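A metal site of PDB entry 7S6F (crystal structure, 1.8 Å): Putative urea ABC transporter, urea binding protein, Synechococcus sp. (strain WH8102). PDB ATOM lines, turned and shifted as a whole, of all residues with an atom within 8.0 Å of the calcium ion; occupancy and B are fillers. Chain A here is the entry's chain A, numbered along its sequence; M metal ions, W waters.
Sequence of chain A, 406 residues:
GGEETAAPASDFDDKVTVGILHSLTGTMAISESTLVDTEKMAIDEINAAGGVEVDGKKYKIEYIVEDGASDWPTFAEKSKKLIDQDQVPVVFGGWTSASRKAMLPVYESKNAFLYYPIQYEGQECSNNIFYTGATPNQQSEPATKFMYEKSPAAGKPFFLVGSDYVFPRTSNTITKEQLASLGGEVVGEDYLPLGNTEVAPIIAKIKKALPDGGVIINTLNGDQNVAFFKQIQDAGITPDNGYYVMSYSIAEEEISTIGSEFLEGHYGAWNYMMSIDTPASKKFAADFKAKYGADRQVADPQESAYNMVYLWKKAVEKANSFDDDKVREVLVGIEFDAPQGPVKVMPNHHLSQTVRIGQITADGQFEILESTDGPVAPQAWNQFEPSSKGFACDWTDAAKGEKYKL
The side-chain amide oxygen (OD1) of Asn 111 is in hydrogen-bond range of the side-chain amide nitrogen (ND2) of Asn 128 (3.0 Å). The side-chain carboxylate (OD2) of Asp 324 is in salt-bridge range of the guanidinium group (NH2) of Arg 328 (2.9 Å). The guanidinium group of Arg 328 sits at hydrogen-bond distance from the side-chain amide oxygen of Asn 111, 3.1 Å away. N of Asp 325 lies within hydrogen-bond range of OD1 of Asp 323 (3.1 Å). The guanidinium group (NH2) of Arg 328 lies close to the side-chain carboxylate (OD1) of Asp 325.
Of the 15 residues printed, 3 come within 4 Å of the calcium ion. The nearest printed residue that does not touch the calcium ion is Ala 112 (4.2 Å).
The calcium ion is bound by water W2, at 2.2 Å. The calcium ion is bound by OD1 of Asp 324 (2.3 Å). The side-chain carboxylate (OD1) of Asp 325 is bound to the calcium ion. The calcium ion is bound by O of Asn 111. Water W1 binds the calcium ion, 2.4 Å away. Water W3 is bound to the calcium ion (2.5 Å). Slightly farther from the calcium ion lies OD2 of Asp 324 (3.0 Å).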
ATOM      1  N   ILE A  83     -26.963 -22.937 -20.299  1.00  0.00           N
ATOM      2  CA  ILE A  83     -27.995 -23.093 -21.366  1.00  0.00           C
ATOM      3  C   ILE A  83     -29.383 -22.820 -20.756  1.00  0.00           C
ATOM      4  O   ILE A  83     -30.108 -21.988 -21.298  1.00  0.00           O
ATOM      5  CB  ILE A  83     -27.910 -24.494 -22.003  1.00  0.00           C
ATOM      6  CG1 ILE A  83     -26.564 -24.708 -22.692  1.00  0.00           C
ATOM      7  CG2 ILE A  83     -29.079 -24.715 -22.957  1.00  0.00           C
ATOM      8  CD1 ILE A  83     -26.359 -26.091 -23.157  1.00  0.00           C
ATOM      9  N   VAL A  88     -28.006 -18.290 -22.005  1.00  0.00           N
ATOM     10  CA  VAL A  88     -26.996 -17.628 -22.867  1.00  0.00           C
ATOM     11  C   VAL A  88     -27.222 -18.117 -24.288  1.00  0.00           C
ATOM     12  O   VAL A  88     -27.630 -19.247 -24.542  1.00  0.00           O
ATOM     13  CB  VAL A  88     -25.560 -17.910 -22.379  1.00  0.00           C
ATOM     14  CG1 VAL A  88     -25.341 -17.424 -20.951  1.00  0.00           C
ATOM     15  CG2 VAL A  88     -25.233 -19.393 -22.510  1.00  0.00           C
ATOM     16  N   PRO A  89     -27.005 -17.252 -25.288  1.00  0.00           N
ATOM     17  CA  PRO A  89     -27.102 -17.654 -26.696  1.00  0.00           C
ATOM     18  C   PRO A  89     -25.891 -18.386 -27.295  1.00  0.00           C
ATOM     19  O   PRO A  89     -25.989 -18.946 -28.362  1.00  0.00           O
ATOM     20  CB  PRO A  89     -27.248 -16.304 -27.407  1.00  0.00           C
ATOM     21  CG  PRO A  89     -26.597 -15.297 -26.509  1.00  0.00           C
ATOM     22  CD  PRO A  89     -26.662 -15.831 -25.097  1.00  0.00           C
ATOM     23  N   TYR A 107     -25.199 -30.141 -25.393  1.00  0.00           N
ATOM     24  CA  TYR A 107     -25.463 -29.168 -26.488  1.00  0.00           C
ATOM     25  C   TYR A 107     -26.348 -29.798 -27.574  1.00  0.00           C
ATOM     26  O   TYR A 107     -27.215 -29.091 -28.100  1.00  0.00           O
ATOM     27  CB  TYR A 107     -24.139 -28.599 -27.006  1.00  0.00           C
ATOM     28  CG  TYR A 107     -23.488 -27.728 -25.975  1.00  0.00           C
ATOM     29  CD1 TYR A 107     -23.834 -26.395 -25.847  1.00  0.00           C
ATOM     30  CD2 TYR A 107     -22.608 -28.263 -25.034  1.00  0.00           C
ATOM     31  CE1 TYR A 107     -23.275 -25.594 -24.874  1.00  0.00           C
ATOM     32  CE2 TYR A 107     -22.028 -27.473 -24.058  1.00  0.00           C
ATOM     33  CZ  TYR A 107     -22.380 -26.136 -23.967  1.00  0.00           C
ATOM     34  OH  TYR A 107     -21.863 -25.348 -22.999  1.00  0.00           O
ATOM     35  N   LYS A 110     -30.205 -30.423 -26.157  1.00  0.00           N
ATOM     36  CA  LYS A 110     -30.953 -29.148 -25.950  1.00  0.00           C
ATOM     37  C   LYS A 110     -30.946 -28.297 -27.233  1.00  0.00           C
ATOM     38  O   LYS A 110     -31.490 -27.176 -27.164  1.00  0.00           O
ATOM     39  CB  LYS A 110     -30.332 -28.373 -24.797  1.00  0.00           C
ATOM     40  CG  LYS A 110     -30.507 -29.071 -23.463  1.00  0.00           C
ATOM     41  CD  LYS A 110     -29.616 -28.521 -22.395  1.00  0.00           C
ATOM     42  CE  LYS A 110     -29.686 -29.392 -21.176  1.00  0.00           C
ATOM     43  NZ  LYS A 110     -31.073 -29.430 -20.659  1.00  0.00           N
ATOM     44  N   ASN A 111     -30.311 -28.787 -28.309  1.00  0.00           N
ATOM     45  CA  ASN A 111     -30.112 -28.094 -29.604  1.00  0.00           C
ATOM     46  C   ASN A 111     -29.566 -26.704 -29.286  1.00  0.00           C
ATOM     47  O   ASN A 111     -30.210 -25.715 -29.659  1.00  0.00           O
ATOM     48  CB  ASN A 111     -31.411 -28.035 -30.400  1.00  0.00           C
ATOM     49  CG  ASN A 111     -31.220 -27.534 -31.817  1.00  0.00           C
ATOM     50  OD1 ASN A 111     -30.172 -27.758 -32.430  1.00  0.00           O
ATOM     51  ND2 ASN A 111     -32.238 -26.916 -32.365  1.00  0.00           N
ATOM     52  N   ALA A 112     -28.411 -26.662 -28.612  1.00  0.00           N
ATOM     53  CA  ALA A 112     -27.775 -25.412 -28.140  1.00  0.00           C
ATOM     54  C   ALA A 112     -26.490 -25.177 -28.949  1.00  0.00           C
ATOM     55  O   ALA A 112     -26.379 -25.685 -30.091  1.00  0.00           O
ATOM     56  CB  ALA A 112     -27.535 -25.522 -26.664  1.00  0.00           C
ATOM     57  N   PHE A 113     -25.534 -24.406 -28.388  1.00  0.00           N
ATOM     58  CA  PHE A 113     -24.381 -23.881 -29.148  1.00  0.00           C
ATOM     59  C   PHE A 113     -23.148 -23.721 -28.233  1.00  0.00           C
ATOM     60  O   PHE A 113     -23.071 -22.804 -27.384  1.00  0.00           O
ATOM     61  CB  PHE A 113     -24.800 -22.608 -29.882  1.00  0.00           C
ATOM     62  CG  PHE A 113     -23.738 -21.938 -30.731  1.00  0.00           C
ATOM     63  CD1 PHE A 113     -22.591 -22.613 -31.119  1.00  0.00           C
ATOM     64  CD2 PHE A 113     -23.900 -20.630 -31.135  1.00  0.00           C
ATOM     65  CE1 PHE A 113     -21.615 -21.969 -31.871  1.00  0.00           C
ATOM     66  CE2 PHE A 113     -22.938 -20.011 -31.929  1.00  0.00           C
ATOM     67  CZ  PHE A 113     -21.773 -20.656 -32.253  1.00  0.00           C
ATOM     68  N   ASN A 128     -24.096 -28.717 -33.274  1.00  0.00           N
ATOM     69  CA  ASN A 128     -24.274 -27.816 -32.101  1.00  0.00           C
ATOM     70  C   ASN A 128     -22.920 -27.265 -31.608  1.00  0.00           C
ATOM     71  O   ASN A 128     -22.924 -26.556 -30.561  1.00  0.00           O
ATOM     72  CB  ASN A 128     -25.069 -28.549 -31.009  1.00  0.00           C
ATOM     73  CG  ASN A 128     -26.433 -28.871 -31.569  1.00  0.00           C
ATOM     74  OD1 ASN A 128     -26.694 -29.983 -31.998  1.00  0.00           O
ATOM     75  ND2 ASN A 128     -27.250 -27.857 -31.681  1.00  0.00           N
ATOM     76  N   PHE A 322     -29.982 -13.235 -31.831  1.00  0.00           N
ATOM     77  CA  PHE A 322     -29.083 -13.970 -30.907  1.00  0.00           C
ATOM     78  C   PHE A 322     -29.459 -15.450 -30.850  1.00  0.00           C
ATOM     79  O   PHE A 322     -28.663 -16.214 -30.274  1.00  0.00           O
ATOM     80  CB  PHE A 322     -29.100 -13.324 -29.531  1.00  0.00           C
ATOM     81  CG  PHE A 322     -28.533 -11.933 -29.503  1.00  0.00           C
ATOM     82  CD1 PHE A 322     -27.166 -11.728 -29.579  1.00  0.00           C
ATOM     83  CD2 PHE A 322     -29.355 -10.827 -29.290  1.00  0.00           C
ATOM     84  CE1 PHE A 322     -26.629 -10.451 -29.485  1.00  0.00           C
ATOM     85  CE2 PHE A 322     -28.818  -9.543 -29.240  1.00  0.00           C
ATOM     86  CZ  PHE A 322     -27.461  -9.359 -29.338  1.00  0.00           C
ATOM     87  N   ASP A 323     -30.625 -15.839 -31.368  1.00  0.00           N
ATOM     88  CA  ASP A 323     -31.099 -17.256 -31.277  1.00  0.00           C
ATOM     89  C   ASP A 323     -30.037 -18.140 -31.960  1.00  0.00           C
ATOM     90  O   ASP A 323     -29.768 -17.996 -33.145  1.00  0.00           O
ATOM     91  CB  ASP A 323     -32.538 -17.373 -31.798  1.00  0.00           C
ATOM     92  CG  ASP A 323     -33.088 -18.802 -31.937  1.00  0.00           C
ATOM     93  OD1 ASP A 323     -32.442 -19.781 -31.478  1.00  0.00           O
ATOM     94  OD2 ASP A 323     -34.146 -18.928 -32.517  1.00  0.00           O
ATOM     95  N   ASP A 324     -29.424 -19.033 -31.195  1.00  0.00           N
ATOM     96  CA  ASP A 324     -28.341 -19.918 -31.683  1.00  0.00           C
ATOM     97  C   ASP A 324     -28.801 -20.747 -32.891  1.00  0.00           C
ATOM     98  O   ASP A 324     -27.971 -21.052 -33.721  1.00  0.00           O
ATOM     99  CB  ASP A 324     -27.845 -20.795 -30.505  1.00  0.00           C
ATOM    100  CG  ASP A 324     -28.784 -21.944 -30.206  1.00  0.00           C
ATOM    101  OD1 ASP A 324     -29.790 -21.697 -29.503  1.00  0.00           O
ATOM    102  OD2 ASP A 324     -28.516 -23.064 -30.703  1.00  0.00           O
ATOM    103  N   ASP A 325     -30.087 -21.100 -33.005  1.00  0.00           N
ATOM    104  CA  ASP A 325     -30.608 -21.877 -34.159  1.00  0.00           C
ATOM    105  C   ASP A 325     -30.327 -21.114 -35.454  1.00  0.00           C
ATOM    106  O   ASP A 325     -29.883 -21.747 -36.419  1.00  0.00           O
ATOM    107  CB  ASP A 325     -32.093 -22.175 -34.009  1.00  0.00           C
ATOM    108  CG  ASP A 325     -32.421 -23.111 -32.870  1.00  0.00           C
ATOM    109  OD1 ASP A 325     -31.519 -23.388 -32.008  1.00  0.00           O
ATOM    110  OD2 ASP A 325     -33.569 -23.505 -32.822  1.00  0.00           O
ATOM    111  N   LYS A 326     -30.487 -19.794 -35.458  1.00  0.00           N
ATOM    112  CA  LYS A 326     -30.274 -18.931 -36.652  1.00  0.00           C
ATOM    113  C   LYS A 326     -28.778 -18.576 -36.761  1.00  0.00           C
ATOM    114  O   LYS A 326     -28.213 -18.601 -37.865  1.00  0.00           O
ATOM    115  CB  LYS A 326     -31.173 -17.705 -36.526  1.00  0.00           C
ATOM    116  CG  LYS A 326     -31.129 -16.777 -37.729  1.00  0.00           C
ATOM    117  CD  LYS A 326     -31.819 -17.310 -38.944  1.00  0.00           C
ATOM    118  CE  LYS A 326     -32.731 -16.270 -39.554  1.00  0.00           C
ATOM    119  NZ  LYS A 326     -33.137 -16.670 -40.923  1.00  0.00           N
ATOM    120  N   ARG A 328     -26.129 -20.243 -35.824  1.00  0.00           N
ATOM    121  CA  ARG A 328     -25.390 -21.446 -36.271  1.00  0.00           C
ATOM    122  C   ARG A 328     -25.587 -21.616 -37.780  1.00  0.00           C
ATOM    123  O   ARG A 328     -24.608 -21.960 -38.483  1.00  0.00           O
ATOM    124  CB  ARG A 328     -25.814 -22.695 -35.474  1.00  0.00           C
ATOM    125  CG  ARG A 328     -25.178 -22.764 -34.091  1.00  0.00           C
ATOM    126  CD  ARG A 328     -25.396 -24.080 -33.386  1.00  0.00           C
ATOM    127  NE  ARG A 328     -26.771 -24.205 -32.886  1.00  0.00           N
ATOM    128  CZ  ARG A 328     -27.728 -24.951 -33.419  1.00  0.00           C
ATOM    129  NH1 ARG A 328     -27.524 -25.688 -34.497  1.00  0.00           N
ATOM    130  NH2 ARG A 328     -28.918 -24.997 -32.849  1.00  0.00           N
HETATM  131 CA    CA M   1     -31.226 -23.525 -29.624  1.00  0.00          CA
HETATM  132  O   HOH W   1     -32.871 -21.751 -29.581  1.00  0.00           O
HETATM  133  O   HOH W   2     -32.821 -24.850 -28.909  1.00  0.00           O
HETATM  134  O   HOH W   3     -30.666 -23.601 -27.231  1.00  0.00           O
